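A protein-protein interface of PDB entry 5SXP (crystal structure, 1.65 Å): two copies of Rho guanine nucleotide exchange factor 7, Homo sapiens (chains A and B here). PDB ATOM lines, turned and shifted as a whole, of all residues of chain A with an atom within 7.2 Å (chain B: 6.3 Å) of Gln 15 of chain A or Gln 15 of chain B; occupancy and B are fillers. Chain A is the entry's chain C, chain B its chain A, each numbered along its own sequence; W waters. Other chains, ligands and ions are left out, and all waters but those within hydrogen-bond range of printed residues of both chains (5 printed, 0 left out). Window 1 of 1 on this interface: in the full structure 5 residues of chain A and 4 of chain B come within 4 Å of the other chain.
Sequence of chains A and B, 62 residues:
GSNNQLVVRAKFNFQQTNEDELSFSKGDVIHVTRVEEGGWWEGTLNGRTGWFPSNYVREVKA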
ATOM      1  N   ASN A  13      -6.224  18.818 -21.473  1.00  0.00           N
ATOM      2  CA  ASN A  13      -6.500  17.442 -21.849  1.00  0.00           C
ATOM      3  C   ASN A  13      -6.372  17.271 -23.358  1.00  0.00           C
ATOM      4  O   ASN A  13      -6.645  18.190 -24.135  1.00  0.00           O
ATOM      5  CB  ASN A  13      -7.906  17.037 -21.395  1.00  0.00           C
ATOM      6  CG  ASN A  13      -8.124  17.211 -19.893  1.00  0.00           C
ATOM      7  OD1 ASN A  13      -7.248  16.914 -19.081  1.00  0.00           O
ATOM      8  ND2 ASN A  13      -9.309  17.689 -19.523  1.00  0.00           N
ATOM      9  N   PHE A  14      -5.942  16.078 -23.768  1.00  0.00           N
ATOM     10  CA  PHE A  14      -5.912  15.700 -25.174  1.00  0.00           C
ATOM     11  C   PHE A  14      -6.256  14.224 -25.301  1.00  0.00           C
ATOM     12  O   PHE A  14      -5.805  13.407 -24.496  1.00  0.00           O
ATOM     13  CB  PHE A  14      -4.538  15.982 -25.807  1.00  0.00           C
ATOM     14  CG  PHE A  14      -4.410  15.456 -27.208  1.00  0.00           C
ATOM     15  CD1 PHE A  14      -5.104  16.054 -28.254  1.00  0.00           C
ATOM     16  CD2 PHE A  14      -3.612  14.356 -27.476  1.00  0.00           C
ATOM     17  CE1 PHE A  14      -4.999  15.562 -29.544  1.00  0.00           C
ATOM     18  CE2 PHE A  14      -3.501  13.860 -28.762  1.00  0.00           C
ATOM     19  CZ  PHE A  14      -4.194  14.463 -29.798  1.00  0.00           C
ATOM     20  N   GLN A  15      -7.054  13.884 -26.311  1.00  0.00           N
ATOM     21  CA  GLN A  15      -7.470  12.508 -26.553  1.00  0.00           C
ATOM     22  C   GLN A  15      -6.993  12.044 -27.921  1.00  0.00           C
ATOM     23  O   GLN A  15      -7.259  12.698 -28.935  1.00  0.00           O
ATOM     24  CB  GLN A  15      -8.991  12.369 -26.448  1.00  0.00           C
ATOM     25  CG  GLN A  15      -9.483  12.285 -25.023  1.00  0.00           C
ATOM     26  CD  GLN A  15      -9.106  10.973 -24.367  1.00  0.00           C
ATOM     27  OE1 GLN A  15      -9.380   9.899 -24.902  1.00  0.00           O
ATOM     28  NE2 GLN A  15      -8.458  11.051 -23.212  1.00  0.00           N
ATOM     29  N   GLN A  16      -6.304  10.907 -27.935  1.00  0.00           N
ATOM     30  CA  GLN A  16      -5.795  10.332 -29.171  1.00  0.00           C
ATOM     31  C   GLN A  16      -6.940   9.993 -30.116  1.00  0.00           C
ATOM     32  O   GLN A  16      -8.060   9.706 -29.687  1.00  0.00           O
ATOM     33  CB  GLN A  16      -5.001   9.062 -28.855  1.00  0.00           C
ATOM     34  CG  GLN A  16      -5.882   7.897 -28.379  1.00  0.00           C
ATOM     35  CD  GLN A  16      -5.116   6.606 -28.160  1.00  0.00           C
ATOM     36  OE1 GLN A  16      -3.883   6.572 -28.195  1.00  0.00           O
ATOM     37  NE2 GLN A  16      -5.853   5.531 -27.948  1.00  0.00           N
ATOM     38  N   THR A  17      -6.643  10.006 -31.417  1.00  0.00           N
ATOM     39  CA  THR A  17      -7.543   9.460 -32.428  1.00  0.00           C
ATOM     40  C   THR A  17      -7.061   8.121 -32.963  1.00  0.00           C
ATOM     41  O   THR A  17      -7.723   7.531 -33.821  1.00  0.00           O
ATOM     42  CB  THR A  17      -7.710  10.440 -33.598  1.00  0.00           C
ATOM     43  OG1 THR A  17      -6.468  10.577 -34.302  1.00  0.00           O
ATOM     44  CG2 THR A  17      -8.168  11.797 -33.099  1.00  0.00           C
ATOM     45  N   ASN A  18      -5.917   7.644 -32.487  1.00  0.00           N
ATOM     46  CA  ASN A  18      -5.351   6.358 -32.869  1.00  0.00           C
ATOM     47  C   ASN A  18      -4.146   6.148 -31.969  1.00  0.00           C
ATOM     48  O   ASN A  18      -3.766   7.038 -31.204  1.00  0.00           O
ATOM     49  CB  ASN A  18      -4.957   6.322 -34.348  1.00  0.00           C
ATOM     50  CG  ASN A  18      -3.899   7.343 -34.686  1.00  0.00           C
ATOM     51  OD1 ASN A  18      -2.720   7.154 -34.384  1.00  0.00           O
ATOM     52  ND2 ASN A  18      -4.312   8.438 -35.315  1.00  0.00           N
ATOM     53  N   GLU A  21      -0.946   8.328 -31.364  1.00  0.00           N
ATOM     54  CA  GLU A  21      -1.124   9.569 -30.627  1.00  0.00           C
ATOM     55  C   GLU A  21      -1.294   9.258 -29.145  1.00  0.00           C
ATOM     56  O   GLU A  21      -1.714   8.162 -28.766  1.00  0.00           O
ATOM     57  CB  GLU A  21      -2.323  10.357 -31.179  1.00  0.00           C
ATOM     58  CG  GLU A  21      -2.060  10.844 -32.607  1.00  0.00           C
ATOM     59  CD  GLU A  21      -3.303  11.183 -33.396  1.00  0.00           C
ATOM     60  OE1 GLU A  21      -4.378  11.384 -32.792  1.00  0.00           O
ATOM     61  OE2 GLU A  21      -3.194  11.248 -34.644  1.00  0.00           O
ATOM     62  N   LEU A  22      -0.949  10.237 -28.303  1.00  0.00           N
ATOM     63  CA  LEU A  22      -0.848  10.059 -26.855  1.00  0.00           C
ATOM     64  C   LEU A  22      -1.948  10.855 -26.157  1.00  0.00           C
ATOM     65  O   LEU A  22      -1.940  12.089 -26.197  1.00  0.00           O
ATOM     66  CB  LEU A  22       0.529  10.509 -26.370  1.00  0.00           C
ATOM     67  CG  LEU A  22       0.838  10.324 -24.885  1.00  0.00           C
ATOM     68  CD1 LEU A  22       1.027   8.852 -24.573  1.00  0.00           C
ATOM     69  CD2 LEU A  22       2.069  11.129 -24.493  1.00  0.00           C
ATOM     70  N   SER A  23      -2.873  10.151 -25.501  1.00  0.00           N
ATOM     71  CA  SER A  23      -3.865  10.800 -24.651  1.00  0.00           C
ATOM     72  C   SER A  23      -3.225  11.219 -23.334  1.00  0.00           C
ATOM     73  O   SER A  23      -2.339  10.534 -22.814  1.00  0.00           O
ATOM     74  CB  SER A  23      -5.041   9.864 -24.353  1.00  0.00           C
ATOM     75  OG  SER A  23      -5.668   9.420 -25.534  1.00  0.00           O
ATOM     76  N   PHE A  24      -3.686  12.336 -22.781  1.00  0.00           N
ATOM     77  CA  PHE A  24      -3.263  12.698 -21.438  1.00  0.00           C
ATOM     78  C   PHE A  24      -4.266  13.659 -20.819  1.00  0.00           C
ATOM     79  O   PHE A  24      -5.140  14.214 -21.489  1.00  0.00           O
ATOM     80  CB  PHE A  24      -1.842  13.288 -21.419  1.00  0.00           C
ATOM     81  CG  PHE A  24      -1.605  14.422 -22.391  1.00  0.00           C
ATOM     82  CD1 PHE A  24      -2.244  15.643 -22.247  1.00  0.00           C
ATOM     83  CD2 PHE A  24      -0.675  14.277 -23.412  1.00  0.00           C
ATOM     84  CE1 PHE A  24      -1.995  16.683 -23.129  1.00  0.00           C
ATOM     85  CE2 PHE A  24      -0.418  15.315 -24.291  1.00  0.00           C
ATOM     86  CZ  PHE A  24      -1.081  16.520 -24.149  1.00  0.00           C
ATOM     87  N   SER A  25      -4.124  13.830 -19.507  1.00  0.00           N
ATOM     88  CA  SER A  25      -4.942  14.723 -18.705  1.00  0.00           C
ATOM     89  C   SER A  25      -4.077  15.856 -18.172  1.00  0.00           C
ATOM     90  O   SER A  25      -2.864  15.700 -17.991  1.00  0.00           O
ATOM     91  CB  SER A  25      -5.589  13.977 -17.535  1.00  0.00           C
ATOM     92  OG  SER A  25      -6.297  12.837 -17.986  1.00  0.00           O
ATOM     93  N   PRO A  53      -0.319  17.473 -29.316  1.00  0.00           N
ATOM     94  CA  PRO A  53      -0.113  18.887 -29.680  1.00  0.00           C
ATOM     95  C   PRO A  53       0.886  19.560 -28.748  1.00  0.00           C
ATOM     96  O   PRO A  53       0.725  19.542 -27.526  1.00  0.00           O
ATOM     97  CB  PRO A  53      -1.512  19.502 -29.541  1.00  0.00           C
ATOM     98  CG  PRO A  53      -2.463  18.347 -29.461  1.00  0.00           C
ATOM     99  CD  PRO A  53      -1.689  17.231 -28.832  1.00  0.00           C
ATOM    100  N   TYR A  56      -0.214  22.158 -26.109  1.00  0.00           N
ATOM    101  CA  TYR A  56      -0.992  21.687 -24.970  1.00  0.00           C
ATOM    102  C   TYR A  56      -0.133  21.401 -23.742  1.00  0.00           C
ATOM    103  O   TYR A  56      -0.676  20.983 -22.716  1.00  0.00           O
ATOM    104  CB  TYR A  56      -1.754  20.406 -25.323  1.00  0.00           C
ATOM    105  CG  TYR A  56      -3.057  20.568 -26.082  1.00  0.00           C
ATOM    106  CD1 TYR A  56      -3.182  21.468 -27.134  1.00  0.00           C
ATOM    107  CD2 TYR A  56      -4.157  19.779 -25.767  1.00  0.00           C
ATOM    108  CE1 TYR A  56      -4.378  21.589 -27.836  1.00  0.00           C
ATOM    109  CE2 TYR A  56      -5.349  19.894 -26.462  1.00  0.00           C
ATOM    110  CZ  TYR A  56      -5.454  20.796 -27.494  1.00  0.00           C
ATOM    111  OH  TYR A  56      -6.650  20.895 -28.178  1.00  0.00           O
ATOM    112  N   ASN B  13     -10.342  13.030 -37.956  1.00  0.00           N
ATOM    113  CA  ASN B  13     -10.878  12.538 -36.692  1.00  0.00           C
ATOM    114  C   ASN B  13     -10.609  13.536 -35.573  1.00  0.00           C
ATOM    115  O   ASN B  13      -9.538  14.150 -35.508  1.00  0.00           O
ATOM    116  CB  ASN B  13     -10.242  11.199 -36.313  1.00  0.00           C
ATOM    117  CG  ASN B  13     -10.514  10.110 -37.321  1.00  0.00           C
ATOM    118  OD1 ASN B  13     -11.608  10.006 -37.871  1.00  0.00           O
ATOM    119  ND2 ASN B  13      -9.515   9.274 -37.556  1.00  0.00           N
ATOM    120  N   PHE B  14     -11.580  13.677 -34.674  1.00  0.00           N
ATOM    121  CA  PHE B  14     -11.398  14.478 -33.473  1.00  0.00           C
ATOM    122  C   PHE B  14     -12.077  13.767 -32.318  1.00  0.00           C
ATOM    123  O   PHE B  14     -13.219  13.313 -32.450  1.00  0.00           O
ATOM    124  CB  PHE B  14     -11.968  15.895 -33.630  1.00  0.00           C
ATOM    125  CG  PHE B  14     -11.909  16.700 -32.362  1.00  0.00           C
ATOM    126  CD1 PHE B  14     -10.704  17.205 -31.903  1.00  0.00           C
ATOM    127  CD2 PHE B  14     -13.058  16.942 -31.624  1.00  0.00           C
ATOM    128  CE1 PHE B  14     -10.644  17.935 -30.730  1.00  0.00           C
ATOM    129  CE2 PHE B  14     -13.007  17.675 -30.453  1.00  0.00           C
ATOM    130  CZ  PHE B  14     -11.800  18.171 -30.005  1.00  0.00           C
ATOM    131  N   GLN B  15     -11.376  13.675 -31.193  1.00  0.00           N
ATOM    132  CA  GLN B  15     -11.890  12.999 -30.010  1.00  0.00           C
ATOM    133  C   GLN B  15     -12.050  14.010 -28.882  1.00  0.00           C
ATOM    134  O   GLN B  15     -11.065  14.608 -28.432  1.00  0.00           O
ATOM    135  CB  GLN B  15     -10.959  11.857 -29.594  1.00  0.00           C
ATOM    136  CG  GLN B  15     -11.594  10.860 -28.643  1.00  0.00           C
ATOM    137  CD  GLN B  15     -12.811  10.171 -29.241  1.00  0.00           C
ATOM    138  OE1 GLN B  15     -12.765   9.648 -30.358  1.00  0.00           O
ATOM    139  NE2 GLN B  15     -13.905  10.171 -28.500  1.00  0.00           N
ATOM    140  N   GLN B  16     -13.289  14.184 -28.421  1.00  0.00           N
ATOM    141  CA  GLN B  16     -13.586  15.165 -27.389  1.00  0.00           C
ATOM    142  C   GLN B  16     -12.839  14.830 -26.101  1.00  0.00           C
ATOM    143  O   GLN B  16     -12.558  13.666 -25.802  1.00  0.00           O
ATOM    144  CB  GLN B  16     -15.093  15.204 -27.125  1.00  0.00           C
ATOM    145  CG  GLN B  16     -15.604  14.012 -26.336  1.00  0.00           C
ATOM    146  CD  GLN B  16     -17.100  13.810 -26.482  1.00  0.00           C
ATOM    147  OE1 GLN B  16     -17.565  13.178 -27.428  1.00  0.00           O
ATOM    148  NE2 GLN B  16     -17.862  14.343 -25.541  1.00  0.00           N
ATOM    149  N   THR B  17     -12.520  15.871 -25.332  1.00  0.00           N
ATOM    150  CA  THR B  17     -11.908  15.704 -24.020  1.00  0.00           C
ATOM    151  C   THR B  17     -12.874  15.975 -22.878  1.00  0.00           C
ATOM    152  O   THR B  17     -12.545  15.670 -21.725  1.00  0.00           O
ATOM    153  CB  THR B  17     -10.682  16.621 -23.871  1.00  0.00           C
ATOM    154  OG1 THR B  17     -11.097  17.991 -23.798  1.00  0.00           O
ATOM    155  CG2 THR B  17      -9.733  16.447 -25.042  1.00  0.00           C
ATOM    156  N   GLU B  21     -17.418  19.269 -25.935  1.00  0.00           N
ATOM    157  CA  GLU B  21     -16.814  19.099 -27.244  1.00  0.00           C
ATOM    158  C   GLU B  21     -17.483  17.945 -27.981  1.00  0.00           C
ATOM    159  O   GLU B  21     -18.055  17.037 -27.374  1.00  0.00           O
ATOM    160  CB  GLU B  21     -15.305  18.852 -27.114  1.00  0.00           C
ATOM    161  CG  GLU B  21     -14.524  20.081 -26.647  1.00  0.00           C
ATOM    162  CD  GLU B  21     -13.073  19.785 -26.274  1.00  0.00           C
ATOM    163  OE1 GLU B  21     -12.688  18.600 -26.219  1.00  0.00           O
ATOM    164  OE2 GLU B  21     -12.314  20.748 -26.030  1.00  0.00           O
ATOM    165  N   LEU B  22     -17.404  17.998 -29.306  1.00  0.00           N
ATOM    166  CA  LEU B  22     -18.075  17.047 -30.186  1.00  0.00           C
ATOM    167  C   LEU B  22     -17.041  16.144 -30.849  1.00  0.00           C
ATOM    168  O   LEU B  22     -16.178  16.629 -31.587  1.00  0.00           O
ATOM    169  CB  LEU B  22     -18.887  17.792 -31.245  1.00  0.00           C
ATOM    170  CG  LEU B  22     -19.780  16.979 -32.177  1.00  0.00           C
ATOM    171  CD1 LEU B  22     -21.006  16.478 -31.434  1.00  0.00           C
ATOM    172  CD2 LEU B  22     -20.176  17.825 -33.366  1.00  0.00           C
ATOM    173  N   SER B  23     -17.140  14.838 -30.596  1.00  0.00           N
ATOM    174  CA  SER B  23     -16.287  13.859 -31.261  1.00  0.00           C
ATOM    175  C   SER B  23     -16.833  13.527 -32.644  1.00  0.00           C
ATOM    176  O   SER B  23     -18.047  13.526 -32.867  1.00  0.00           O
ATOM    177  CB  SER B  23     -16.203  12.562 -30.452  1.00  0.00           C
ATOM    178  OG  SER B  23     -15.581  12.760 -29.202  1.00  0.00           O
ATOM    179  N   PHE B  24     -15.926  13.218 -33.573  1.00  0.00           N
ATOM    180  CA  PHE B  24     -16.365  12.683 -34.855  1.00  0.00           C
ATOM    181  C   PHE B  24     -15.239  11.943 -35.562  1.00  0.00           C
ATOM    182  O   PHE B  24     -14.058  12.076 -35.224  1.00  0.00           O
ATOM    183  CB  PHE B  24     -16.932  13.775 -35.775  1.00  0.00           C
ATOM    184  CG  PHE B  24     -16.090  15.029 -35.879  1.00  0.00           C
ATOM    185  CD1 PHE B  24     -14.846  15.021 -36.491  1.00  0.00           C
ATOM    186  CD2 PHE B  24     -16.587  16.234 -35.406  1.00  0.00           C
ATOM    187  CE1 PHE B  24     -14.106  16.192 -36.604  1.00  0.00           C
ATOM    188  CE2 PHE B  24     -15.863  17.405 -35.520  1.00  0.00           C
ATOM    189  CZ  PHE B  24     -14.618  17.388 -36.114  1.00  0.00           C
HETATM  190  O   HOH W   1      -8.439  14.505 -30.688  1.00  0.00           O
HETATM  191  O   HOH W   2     -11.157  18.894 -21.140  1.00  0.00           O
HETATM  192  O   HOH W   3      -6.742  10.065 -37.019  1.00  0.00           O
HETATM  193  O   HOH W   4      -8.564  15.871 -28.272  1.00  0.00           O
HETATM  194  O   HOH W   5     -10.591   8.263 -31.501  1.00  0.00           O
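The side-chain amide oxygen (OE1) of Gln 16 of chain A lies close to the backbone carbonyl oxygen (O) of Glu 21 of chain A. OG1 of Thr 17 of chain A lies within hydrogen-bond range of ND2 of Asn 18 of chain A, at 3.2 Å. NE2 of Gln 16 of chain B lies within hydrogen-bond range of O of Glu 21 of chain B, at 3.3 Å. The side-chain hydroxyl (OG) of Ser 23 of chain A is in hydrogen-bond range of the backbone NH (N) of Gln 16 of chain A, at 2.9 Å. The side-chain hydroxyl of Ser 23 of chain B sits at hydrogen-bond distance from the side-chain amide oxygen of Gln 16 of chain B, at 2.7 Å. The backbone NH (N) of Phe 24 of chain A lies within hydrogen-bond range of the backbone carbonyl oxygen (O) of Phe 14 of chain A, 2.9 Å away.
Thr 17 of chain B touches Asn 13 of chain A. Phe 14 of chain A touches Thr 17 of chain B (CA to CG2, 3.9 Å). Gln 15 of chain A touches Gln 15 of chain B. Gln 15 of chain A touches Gln 16 of chain B. Thr 17 of chain B touches Gln 15 of chain A. Gln 16 of chain A touches Gln 15 of chain B. Asn 13 of chain B touches Thr 17 of chain A (O to CG2, 3.6 Å).
Printed residues of chain B within 4 Å of Phe 14 of chain A: Thr 17. Gln 15 of chain A touches just these residues of chain B: Gln 15, Gln 16 and Thr 17. Of the printed residues of chain B, Gln 16 of chain A touches Gln 15 (3.6 Å). Printed residues of chain A within 4 Å of Asn 13 of chain B: Thr 17 (3.6 Å). Gln 15 of chain B touches two residues of chain A. Printed residues of chain A within 4 Å of Gln 16 of chain B: Gln 15 (3.5 Å). The nearest residue of chain A that does not touch Gln 15 of chain B is Thr 17 of chain A (4.2 Å).
Printed residues of chain B that touch a printed residue of chain A: Asn 13, Gln 15, Gln 16 and Thr 17. Of the 13 printed residues of chain A, 5 touch a printed residue of chain B. Among the printed residues, 7 pairs touch across the chains. Among the printed residues, no Asp or Glu carboxylate lies within 4 Å of a Lys or Arg side-chain nitrogen of the other chain.
Phe 14 of chain A touches Thr 17 of chain B, but with the chains exchanged Thr 17 of chain A does not touch Phe 14 of chain B (4.2 Å). Gln 15 of chain B touches its own counterpart, Gln 15 of chain A. Gln 15 of chain A touches Gln 16 of chain B, and with the chains exchanged Gln 16 of chain A touches Gln 15 of chain B. Gln 15 of chain A touches Thr 17 of chain B, but with the chains exchanged Thr 17 of chain A does not touch Gln 15 of chain B (4.2 Å). Positions printed for both chains: 13, 14, 15, 16, 17, 21, 22, 23 and 24. Of the 7 pairs that touch across the chains among the printed residues, 5 have their exchanged pair printed and touching as well.
Water W2 lies within hydrogen-bond range of the side-chain amide nitrogen (ND2) of Asn 13 of chain A (2.7 Å) and the side-chain hydroxyl (OG1) of Thr 17 of chain B (2.8 Å). Water W3 lies within hydrogen-bond range of the side-chain hydroxyl (OG1) of Thr 17 of chain A, the side-chain amide nitrogen (ND2) of Asn 13 of chain B and the side-chain amide nitrogen (ND2) of Asn 18 of chain A. Water W1 bridges the backbone carbonyl oxygen of Gln 15 of chain A (2.8 Å) and the backbone NH of Gln 15 of chain B (3.1 Å). Water W4 bridges O of Gln 15 of chain B (2.8 Å) and N of Gln 15 of chain A (3.2 Å). Water W5 bridges OE1 of Gln 15 of chain B (2.8 Å) and O of Gln 16 of chain A (3.4 Å).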
